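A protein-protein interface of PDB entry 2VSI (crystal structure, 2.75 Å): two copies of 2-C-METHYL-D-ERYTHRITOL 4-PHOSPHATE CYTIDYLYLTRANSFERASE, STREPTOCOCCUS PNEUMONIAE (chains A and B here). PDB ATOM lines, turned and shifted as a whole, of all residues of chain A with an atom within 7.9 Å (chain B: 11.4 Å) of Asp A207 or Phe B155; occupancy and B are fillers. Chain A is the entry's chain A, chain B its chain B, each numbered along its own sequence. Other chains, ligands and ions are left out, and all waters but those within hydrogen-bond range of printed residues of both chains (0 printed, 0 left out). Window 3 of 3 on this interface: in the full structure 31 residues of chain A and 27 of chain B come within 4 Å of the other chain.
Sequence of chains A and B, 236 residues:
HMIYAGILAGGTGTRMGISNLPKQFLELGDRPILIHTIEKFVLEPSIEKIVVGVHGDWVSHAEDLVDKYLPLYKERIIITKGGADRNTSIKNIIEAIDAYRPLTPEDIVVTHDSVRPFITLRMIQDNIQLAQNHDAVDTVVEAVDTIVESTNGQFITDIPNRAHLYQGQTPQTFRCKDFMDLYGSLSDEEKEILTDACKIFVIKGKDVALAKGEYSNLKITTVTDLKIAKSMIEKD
Asp A138 touches Val B148 (OD2 to CG2, 3.7 Å).
Asp A138 touches Ile B156.
Tyr A166 touches Ser B150 (CE1 to CB, 3.7 Å).
OD2 of Asp A207 touches CB of Phe B155, at 3.4 Å.
Val A208 touches Phe B155.
Ala A209 touches Gln B154.
Phe B155 touches Ala A209 (CA to CA, 3.99 Å).
CD1 of Leu A210 touches OG of Ser B150, at 3.9 Å.
Leu A210 touches Gly B153 (CD1 to O, 3.7 Å).
Leu A210 touches Ile B156 (CD2 to CG1, 3.6 Å).
The side-chain carboxylate (OD2) of Asp A135 lies within hydrogen-bond range of the backbone NH (N) of Asp A207 (2.9 Å).
The backbone carbonyl oxygen (O) of Ala A136 is in hydrogen-bond range of the backbone NH (N) of Ala A209 (3.2 Å).
O of Ala A209 lies within hydrogen-bond range of N of Asp A138 (2.9 Å).
The backbone NH of Gly B153 lies within hydrogen-bond range of the side-chain hydroxyl of Ser B150, at 3.1 Å.
The side-chain hydroxyl (OG) of Ser B150 lies within hydrogen-bond range of the backbone carbonyl oxygen (O) of Phe B155 (3.0 Å).
N of Gln B154 is in hydrogen-bond range of OD1 of Asn B152, at 2.7 Å.
Hydrophobic or aromatic side chains of chain B that line the printed part of chain A: Val B148, Phe B155 and Ile B156.
Among the printed residues, 13 pairs touch across the chains.
No position is printed for both chains.
The backbone NH (N) of Tyr A166 lies within hydrogen-bond range of the backbone carbonyl oxygen (O) of Val B148, at 2.7 Å.
N of Ile B156 lies within hydrogen-bond range of O of Val A208 (3.0 Å).
The backbone NH (N) of Leu A210 is in hydrogen-bond range of the backbone carbonyl oxygen (O) of Gln B154 (2.9 Å).
No residue of chain B comes within 4 Å of His A134.
Of the printed residues of chain B, Tyr A166 touches Val B148 (2.7 Å) and Ser B150 (3.7 Å).
Lys A206 touches none of the printed residues of chain B.
Asp A207 touches just one residue of chain B: Phe B155 (3.4 Å).
Val A208 touches just these residues of chain B: Phe B155 and Ile B156.
Of the printed residues of chain B, Ala A209 touches Gln B154 (3.1 Å) and Phe B155 (3.99 Å).
Leu A210 touches four residues of chain B.
Printed residues of chain A within 4 Å of Ser B150: Tyr A166 (3.7 Å) and Leu A210 (3.9 Å).
Of the printed residues of chain A, Gln B154 touches Ala A209 and Leu A210.
Of the printed residues of chain A, Ile B156 touches Asp A138 (3.8 Å), Val A208 (3.0 Å) and Leu A210 (3.6 Å).
Thr B157 touches none of the printed residues of chain A.
The nearest printed residue of chain A that does not touch Phe B155 is Leu A210 (4.5 Å).
The nearest printed residue of chain A that does not touch Gly B153 is Tyr A166 (4.01 Å).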
ATOM      1  N   LEU A 130      25.122   6.034  12.605  1.00  0.00           N
ATOM      2  CA  LEU A 130      24.606   5.430  11.372  1.00  0.00           C
ATOM      3  C   LEU A 130      25.489   5.709  10.149  1.00  0.00           C
ATOM      4  O   LEU A 130      25.853   4.775   9.426  1.00  0.00           O
ATOM      5  CB  LEU A 130      23.164   5.877  11.123  1.00  0.00           C
ATOM      6  CG  LEU A 130      21.991   4.938  11.463  1.00  0.00           C
ATOM      7  CD1 LEU A 130      22.356   3.749  12.350  1.00  0.00           C
ATOM      8  CD2 LEU A 130      20.849   5.732  12.077  1.00  0.00           C
ATOM      9  N   ASN A 133      28.347   3.189   8.234  1.00  0.00           N
ATOM     10  CA  ASN A 133      28.124   2.199   7.164  1.00  0.00           C
ATOM     11  C   ASN A 133      26.971   2.537   6.200  1.00  0.00           C
ATOM     12  O   ASN A 133      26.382   1.645   5.582  1.00  0.00           O
ATOM     13  CB  ASN A 133      27.974   0.775   7.749  1.00  0.00           C
ATOM     14  CG  ASN A 133      27.216   0.759   9.076  1.00  0.00           C
ATOM     15  OD1 ASN A 133      26.439   1.678   9.385  1.00  0.00           O
ATOM     16  ND2 ASN A 133      27.442  -0.282   9.872  1.00  0.00           N
ATOM     17  N   HIS A 134      26.657   3.831   6.090  1.00  0.00           N
ATOM     18  CA  HIS A 134      25.722   4.345   5.081  1.00  0.00           C
ATOM     19  C   HIS A 134      26.244   5.643   4.465  1.00  0.00           C
ATOM     20  O   HIS A 134      27.122   6.297   5.031  1.00  0.00           O
ATOM     21  CB  HIS A 134      24.317   4.532   5.670  1.00  0.00           C
ATOM     22  CG  HIS A 134      23.767   3.292   6.308  1.00  0.00           C
ATOM     23  ND1 HIS A 134      23.397   2.179   5.577  1.00  0.00           N
ATOM     24  CD2 HIS A 134      23.552   2.977   7.607  1.00  0.00           C
ATOM     25  CE1 HIS A 134      22.967   1.238   6.397  1.00  0.00           C
ATOM     26  NE2 HIS A 134      23.046   1.699   7.634  1.00  0.00           N
ATOM     27  N   ASP A 135      25.711   5.998   3.298  1.00  0.00           N
ATOM     28  CA  ASP A 135      26.162   7.175   2.554  1.00  0.00           C
ATOM     29  C   ASP A 135      25.711   8.446   3.226  1.00  0.00           C
ATOM     30  O   ASP A 135      26.455   9.433   3.263  1.00  0.00           O
ATOM     31  CB  ASP A 135      25.657   7.126   1.110  1.00  0.00           C
ATOM     32  CG  ASP A 135      26.171   5.916   0.369  1.00  0.00           C
ATOM     33  OD1 ASP A 135      27.409   5.744   0.318  1.00  0.00           O
ATOM     34  OD2 ASP A 135      25.346   5.132  -0.148  1.00  0.00           O
ATOM     35  N   ALA A 136      24.490   8.399   3.754  1.00  0.00           N
ATOM     36  CA  ALA A 136      23.882   9.523   4.449  1.00  0.00           C
ATOM     37  C   ALA A 136      22.774   9.046   5.396  1.00  0.00           C
ATOM     38  O   ALA A 136      22.356   7.883   5.339  1.00  0.00           O
ATOM     39  CB  ALA A 136      23.342  10.521   3.456  1.00  0.00           C
ATOM     40  N   VAL A 137      22.308   9.946   6.262  1.00  0.00           N
ATOM     41  CA  VAL A 137      21.370   9.606   7.323  1.00  0.00           C
ATOM     42  C   VAL A 137      20.273  10.668   7.441  1.00  0.00           C
ATOM     43  O   VAL A 137      20.570  11.855   7.590  1.00  0.00           O
ATOM     44  CB  VAL A 137      22.094   9.512   8.689  1.00  0.00           C
ATOM     45  CG1 VAL A 137      21.200   8.869   9.742  1.00  0.00           C
ATOM     46  CG2 VAL A 137      23.366   8.732   8.564  1.00  0.00           C
ATOM     47  N   ASP A 138      19.015  10.233   7.391  1.00  0.00           N
ATOM     48  CA  ASP A 138      17.874  11.135   7.549  1.00  0.00           C
ATOM     49  C   ASP A 138      17.207  10.881   8.891  1.00  0.00           C
ATOM     50  O   ASP A 138      17.044   9.726   9.287  1.00  0.00           O
ATOM     51  CB  ASP A 138      16.853  10.952   6.410  1.00  0.00           C
ATOM     52  CG  ASP A 138      16.068  12.238   6.095  1.00  0.00           C
ATOM     53  OD1 ASP A 138      16.275  13.268   6.772  1.00  0.00           O
ATOM     54  OD2 ASP A 138      15.247  12.225   5.143  1.00  0.00           O
ATOM     55  N   TYR A 166       6.847   8.743   6.365  1.00  0.00           N
ATOM     56  CA  TYR A 166       7.539   9.284   7.513  1.00  0.00           C
ATOM     57  C   TYR A 166       7.543  10.792   7.417  1.00  0.00           C
ATOM     58  O   TYR A 166       7.674  11.362   6.329  1.00  0.00           O
ATOM     59  CB  TYR A 166       8.977   8.758   7.554  1.00  0.00           C
ATOM     60  CG  TYR A 166       9.060   7.273   7.788  1.00  0.00           C
ATOM     61  CD1 TYR A 166       9.002   6.375   6.726  1.00  0.00           C
ATOM     62  CD2 TYR A 166       9.176   6.764   9.075  1.00  0.00           C
ATOM     63  CE1 TYR A 166       9.064   4.994   6.944  1.00  0.00           C
ATOM     64  CE2 TYR A 166       9.239   5.390   9.302  1.00  0.00           C
ATOM     65  CZ  TYR A 166       9.183   4.518   8.233  1.00  0.00           C
ATOM     66  OH  TYR A 166       9.249   3.173   8.465  1.00  0.00           O
ATOM     67  N   THR A 173      22.630  13.830   7.979  1.00  0.00           N
ATOM     68  CA  THR A 173      24.035  13.628   8.201  1.00  0.00           C
ATOM     69  C   THR A 173      24.595  12.805   7.047  1.00  0.00           C
ATOM     70  O   THR A 173      23.979  11.827   6.607  1.00  0.00           O
ATOM     71  CB  THR A 173      24.249  12.931   9.576  1.00  0.00           C
ATOM     72  OG1 THR A 173      23.937  13.857  10.621  1.00  0.00           O
ATOM     73  CG2 THR A 173      25.689  12.407   9.776  1.00  0.00           C
ATOM     74  N   ARG A 175      28.707  12.520   4.562  1.00  0.00           N
ATOM     75  CA  ARG A 175      30.066  12.994   4.309  1.00  0.00           C
ATOM     76  C   ARG A 175      30.064  14.312   3.521  1.00  0.00           C
ATOM     77  O   ARG A 175      29.087  14.642   2.846  1.00  0.00           O
ATOM     78  CB  ARG A 175      30.871  11.909   3.608  1.00  0.00           C
ATOM     79  CG  ARG A 175      31.154  10.741   4.537  1.00  0.00           C
ATOM     80  CD  ARG A 175      31.523   9.463   3.802  1.00  0.00           C
ATOM     81  NE  ARG A 175      31.606   8.319   4.713  1.00  0.00           N
ATOM     82  CZ  ARG A 175      30.562   7.610   5.140  1.00  0.00           C
ATOM     83  NH1 ARG A 175      29.330   7.920   4.748  1.00  0.00           N
ATOM     84  NH2 ARG A 175      30.749   6.579   5.958  1.00  0.00           N
ATOM     85  N   PHE A 201      20.722  12.629  -2.506  1.00  0.00           N
ATOM     86  CA  PHE A 201      21.361  11.325  -2.290  1.00  0.00           C
ATOM     87  C   PHE A 201      20.520  10.154  -2.810  1.00  0.00           C
ATOM     88  O   PHE A 201      21.062   9.184  -3.326  1.00  0.00           O
ATOM     89  CB  PHE A 201      21.690  11.120  -0.799  1.00  0.00           C
ATOM     90  CG  PHE A 201      22.993  11.753  -0.360  1.00  0.00           C
ATOM     91  CD1 PHE A 201      23.066  13.126  -0.076  1.00  0.00           C
ATOM     92  CD2 PHE A 201      24.144  10.978  -0.221  1.00  0.00           C
ATOM     93  CE1 PHE A 201      24.272  13.712   0.333  1.00  0.00           C
ATOM     94  CE2 PHE A 201      25.348  11.552   0.187  1.00  0.00           C
ATOM     95  CZ  PHE A 201      25.415  12.919   0.466  1.00  0.00           C
ATOM     96  N   VAL A 202      19.200  10.256  -2.679  1.00  0.00           N
ATOM     97  CA  VAL A 202      18.298   9.174  -3.078  1.00  0.00           C
ATOM     98  C   VAL A 202      18.229   9.046  -4.599  1.00  0.00           C
ATOM     99  O   VAL A 202      18.399   7.956  -5.140  1.00  0.00           O
ATOM    100  CB  VAL A 202      16.873   9.366  -2.505  1.00  0.00           C
ATOM    101  CG1 VAL A 202      16.051   8.095  -2.681  1.00  0.00           C
ATOM    102  CG2 VAL A 202      16.927   9.765  -1.026  1.00  0.00           C
ATOM    103  N   LYS A 204      20.314   9.979  -6.750  1.00  0.00           N
ATOM    104  CA  LYS A 204      21.600   9.520  -7.260  1.00  0.00           C
ATOM    105  C   LYS A 204      21.844   8.073  -6.851  1.00  0.00           C
ATOM    106  O   LYS A 204      22.961   7.575  -6.944  1.00  0.00           O
ATOM    107  CB  LYS A 204      22.742  10.440  -6.805  1.00  0.00           C
ATOM    108  CG  LYS A 204      22.774  11.813  -7.496  1.00  0.00           C
ATOM    109  CD  LYS A 204      22.963  11.718  -9.037  1.00  0.00           C
ATOM    110  CE  LYS A 204      22.977  13.118  -9.687  1.00  0.00           C
ATOM    111  NZ  LYS A 204      22.668  13.118 -11.153  1.00  0.00           N
ATOM    112  N   GLY A 205      20.779   7.411  -6.403  1.00  0.00           N
ATOM    113  CA  GLY A 205      20.789   5.982  -6.111  1.00  0.00           C
ATOM    114  C   GLY A 205      21.649   5.588  -4.931  1.00  0.00           C
ATOM    115  O   GLY A 205      22.277   4.533  -4.943  1.00  0.00           O
ATOM    116  N   LYS A 206      21.664   6.429  -3.902  1.00  0.00           N
ATOM    117  CA  LYS A 206      22.538   6.205  -2.754  1.00  0.00           C
ATOM    118  C   LYS A 206      21.787   5.723  -1.508  1.00  0.00           C
ATOM    119  O   LYS A 206      20.624   6.068  -1.295  1.00  0.00           O
ATOM    120  CB  LYS A 206      23.389   7.452  -2.465  1.00  0.00           C
ATOM    121  CG  LYS A 206      24.117   7.980  -3.703  1.00  0.00           C
ATOM    122  CD  LYS A 206      25.510   8.499  -3.384  1.00  0.00           C
ATOM    123  CE  LYS A 206      26.393   8.540  -4.635  1.00  0.00           C
ATOM    124  NZ  LYS A 206      26.796   7.179  -5.095  1.00  0.00           N
ATOM    125  N   ASP A 207      22.474   4.909  -0.705  1.00  0.00           N
ATOM    126  CA  ASP A 207      21.926   4.307   0.511  1.00  0.00           C
ATOM    127  C   ASP A 207      21.775   5.333   1.633  1.00  0.00           C
ATOM    128  O   ASP A 207      22.770   5.714   2.257  1.00  0.00           O
ATOM    129  CB  ASP A 207      22.836   3.151   0.952  1.00  0.00           C
ATOM    130  CG  ASP A 207      22.386   2.490   2.248  1.00  0.00           C
ATOM    131  OD1 ASP A 207      23.173   1.666   2.775  1.00  0.00           O
ATOM    132  OD2 ASP A 207      21.263   2.773   2.739  1.00  0.00           O
ATOM    133  N   VAL A 208      20.535   5.769   1.883  1.00  0.00           N
ATOM    134  CA  VAL A 208      20.225   6.716   2.975  1.00  0.00           C
ATOM    135  C   VAL A 208      19.374   6.057   4.062  1.00  0.00           C
ATOM    136  O   VAL A 208      18.159   5.866   3.889  1.00  0.00           O
ATOM    137  CB  VAL A 208      19.487   7.991   2.475  1.00  0.00           C
ATOM    138  CG1 VAL A 208      19.196   8.945   3.631  1.00  0.00           C
ATOM    139  CG2 VAL A 208      20.304   8.700   1.428  1.00  0.00           C
ATOM    140  N   ALA A 209      20.016   5.726   5.181  1.00  0.00           N
ATOM    141  CA  ALA A 209      19.334   5.096   6.301  1.00  0.00           C
ATOM    142  C   ALA A 209      18.569   6.124   7.138  1.00  0.00           C
ATOM    143  O   ALA A 209      18.796   7.334   7.027  1.00  0.00           O
ATOM    144  CB  ALA A 209      20.317   4.325   7.153  1.00  0.00           C
ATOM    145  N   LEU A 210      17.666   5.617   7.976  1.00  0.00           N
ATOM    146  CA  LEU A 210      16.801   6.440   8.815  1.00  0.00           C
ATOM    147  C   LEU A 210      17.273   6.470  10.269  1.00  0.00           C
ATOM    148  O   LEU A 210      17.626   5.444  10.843  1.00  0.00           O
ATOM    149  CB  LEU A 210      15.363   5.908   8.772  1.00  0.00           C
ATOM    150  CG  LEU A 210      14.734   5.528   7.430  1.00  0.00           C
ATOM    151  CD1 LEU A 210      13.464   4.731   7.655  1.00  0.00           C
ATOM    152  CD2 LEU A 210      14.462   6.761   6.589  1.00  0.00           C
ATOM    153  N   VAL B 148       8.742  11.501   3.723  1.00  0.00           N
ATOM    154  CA  VAL B 148       9.767  10.548   3.323  1.00  0.00           C
ATOM    155  C   VAL B 148       9.160   9.157   3.258  1.00  0.00           C
ATOM    156  O   VAL B 148       8.560   8.684   4.225  1.00  0.00           O
ATOM    157  CB  VAL B 148      10.953  10.547   4.321  1.00  0.00           C
ATOM    158  CG1 VAL B 148      12.003   9.523   3.924  1.00  0.00           C
ATOM    159  CG2 VAL B 148      11.578  11.939   4.428  1.00  0.00           C
ATOM    160  N   GLU B 149       9.318   8.501   2.117  1.00  0.00           N
ATOM    161  CA  GLU B 149       8.830   7.148   1.964  1.00  0.00           C
ATOM    162  C   GLU B 149       9.957   6.131   2.136  1.00  0.00           C
ATOM    163  O   GLU B 149      11.068   6.328   1.640  1.00  0.00           O
ATOM    164  CB  GLU B 149       8.149   6.983   0.605  1.00  0.00           C
ATOM    165  CG  GLU B 149       7.150   5.837   0.543  1.00  0.00           C
ATOM    166  CD  GLU B 149       6.656   5.572  -0.864  1.00  0.00           C
ATOM    167  OE1 GLU B 149       5.481   5.906  -1.145  1.00  0.00           O
ATOM    168  OE2 GLU B 149       7.443   5.039  -1.682  1.00  0.00           O
ATOM    169  N   SER B 150       9.658   5.051   2.855  1.00  0.00           N
ATOM    170  CA  SER B 150      10.568   3.927   3.003  1.00  0.00           C
ATOM    171  C   SER B 150       9.751   2.655   3.109  1.00  0.00           C
ATOM    172  O   SER B 150       9.044   2.441   4.097  1.00  0.00           O
ATOM    173  CB  SER B 150      11.451   4.094   4.241  1.00  0.00           C
ATOM    174  OG  SER B 150      12.257   2.944   4.446  1.00  0.00           O
ATOM    175  N   THR B 151       9.849   1.816   2.082  1.00  0.00           N
ATOM    176  CA  THR B 151       9.096   0.559   2.029  1.00  0.00           C
ATOM    177  C   THR B 151       9.710  -0.529   2.905  1.00  0.00           C
ATOM    178  O   THR B 151       8.982  -1.323   3.508  1.00  0.00           O
ATOM    179  CB  THR B 151       8.913   0.036   0.577  1.00  0.00           C
ATOM    180  OG1 THR B 151      10.182  -0.346   0.026  1.00  0.00           O
ATOM    181  CG2 THR B 151       8.252   1.105  -0.306  1.00  0.00           C
ATOM    182  N   ASN B 152      11.041  -0.566   2.972  1.00  0.00           N
ATOM    183  CA  ASN B 152      11.738  -1.555   3.803  1.00  0.00           C
ATOM    184  C   ASN B 152      11.754  -1.178   5.289  1.00  0.00           C
ATOM    185  O   ASN B 152      11.574  -2.041   6.151  1.00  0.00           O
ATOM    186  CB  ASN B 152      13.153  -1.851   3.272  1.00  0.00           C
ATOM    187  CG  ASN B 152      14.017  -0.602   3.151  1.00  0.00           C
ATOM    188  OD1 ASN B 152      14.290   0.080   4.139  1.00  0.00           O
ATOM    189  ND2 ASN B 152      14.465  -0.307   1.933  1.00  0.00           N
ATOM    190  N   GLY B 153      11.950   0.109   5.577  1.00  0.00           N
ATOM    191  CA  GLY B 153      11.934   0.607   6.951  1.00  0.00           C
ATOM    192  C   GLY B 153      13.289   0.919   7.573  1.00  0.00           C
ATOM    193  O   GLY B 153      13.365   1.252   8.756  1.00  0.00           O
ATOM    194  N   GLN B 154      14.360   0.807   6.790  1.00  0.00           N
ATOM    195  CA  GLN B 154      15.707   1.125   7.275  1.00  0.00           C
ATOM    196  C   GLN B 154      16.439   2.111   6.378  1.00  0.00           C
ATOM    197  O   GLN B 154      17.230   2.921   6.862  1.00  0.00           O
ATOM    198  CB  GLN B 154      16.535  -0.139   7.492  1.00  0.00           C
ATOM    199  CG  GLN B 154      16.601  -0.563   8.954  1.00  0.00           C
ATOM    200  CD  GLN B 154      16.449  -2.064   9.146  1.00  0.00           C
ATOM    201  OE1 GLN B 154      16.272  -2.812   8.184  1.00  0.00           O
ATOM    202  NE2 GLN B 154      16.507  -2.511  10.397  1.00  0.00           N
ATOM    203  N   PHE B 155      16.184   2.035   5.075  1.00  0.00           N
ATOM    204  CA  PHE B 155      16.666   3.058   4.152  1.00  0.00           C
ATOM    205  C   PHE B 155      15.559   3.507   3.193  1.00  0.00           C
ATOM    206  O   PHE B 155      14.703   2.708   2.808  1.00  0.00           O
ATOM    207  CB  PHE B 155      17.954   2.626   3.422  1.00  0.00           C
ATOM    208  CG  PHE B 155      17.745   1.607   2.330  1.00  0.00           C
ATOM    209  CD1 PHE B 155      17.358   2.004   1.049  1.00  0.00           C
ATOM    210  CD2 PHE B 155      17.965   0.259   2.571  1.00  0.00           C
ATOM    211  CE1 PHE B 155      17.170   1.074   0.036  1.00  0.00           C
ATOM    212  CE2 PHE B 155      17.781  -0.680   1.562  1.00  0.00           C
ATOM    213  CZ  PHE B 155      17.380  -0.272   0.292  1.00  0.00           C
ATOM    214  N   ILE B 156      15.593   4.792   2.835  1.00  0.00           N
ATOM    215  CA  ILE B 156      14.568   5.458   2.017  1.00  0.00           C
ATOM    216  C   ILE B 156      14.366   4.838   0.629  1.00  0.00           C
ATOM    217  O   ILE B 156      15.333   4.484  -0.041  1.00  0.00           O
ATOM    218  CB  ILE B 156      14.936   6.952   1.829  1.00  0.00           C
ATOM    219  CG1 ILE B 156      15.104   7.629   3.194  1.00  0.00           C
ATOM    220  CG2 ILE B 156      13.914   7.677   0.941  1.00  0.00           C
ATOM    221  CD1 ILE B 156      15.614   9.058   3.143  1.00  0.00           C
ATOM    222  N   THR B 157      13.109   4.722   0.202  1.00  0.00           N
ATOM    223  CA  THR B 157      12.794   4.342  -1.176  1.00  0.00           C
ATOM    224  C   THR B 157      12.190   5.486  -2.006  1.00  0.00           C
ATOM    225  O   THR B 157      11.890   5.295  -3.188  1.00  0.00           O
ATOM    226  CB  THR B 157      11.845   3.120  -1.246  1.00  0.00           C
ATOM    227  OG1 THR B 157      10.735   3.319  -0.361  1.00  0.00           O
ATOM    228  CG2 THR B 157      12.585   1.837  -0.878  1.00  0.00           C
ATOM    229  N   ASP B 158      12.012   6.662  -1.399  1.00  0.00           N
ATOM    230  CA  ASP B 158      11.370   7.791  -2.082  1.00  0.00           C
ATOM    231  C   ASP B 158      11.178   9.054  -1.219  1.00  0.00           C
ATOM    232  O   ASP B 158      10.717   8.979  -0.079  1.00  0.00           O
ATOM    233  CB  ASP B 158      10.009   7.344  -2.638  1.00  0.00           C
ATOM    234  CG  ASP B 158       9.427   8.316  -3.649  1.00  0.00           C
ATOM    235  OD1 ASP B 158      10.032   9.379  -3.904  1.00  0.00           O
ATOM    236  OD2 ASP B 158       8.348   8.010  -4.192  1.00  0.00           O
ATOM    237  N   ILE B 159      11.525  10.208  -1.782  1.00  0.00           N
ATOM    238  CA  ILE B 159      11.095  11.493  -1.225  1.00  0.00           C
ATOM    239  C   ILE B 159      10.252  12.217  -2.276  1.00  0.00           C
ATOM    240  O   ILE B 159      10.796  12.871  -3.170  1.00  0.00           O
ATOM    241  CB  ILE B 159      12.271  12.400  -0.748  1.00  0.00           C
ATOM    242  CG1 ILE B 159      13.144  11.669   0.277  1.00  0.00           C
ATOM    243  CG2 ILE B 159      11.720  13.708  -0.143  1.00  0.00           C
ATOM    244  CD1 ILE B 159      14.370  12.428   0.704  1.00  0.00           C
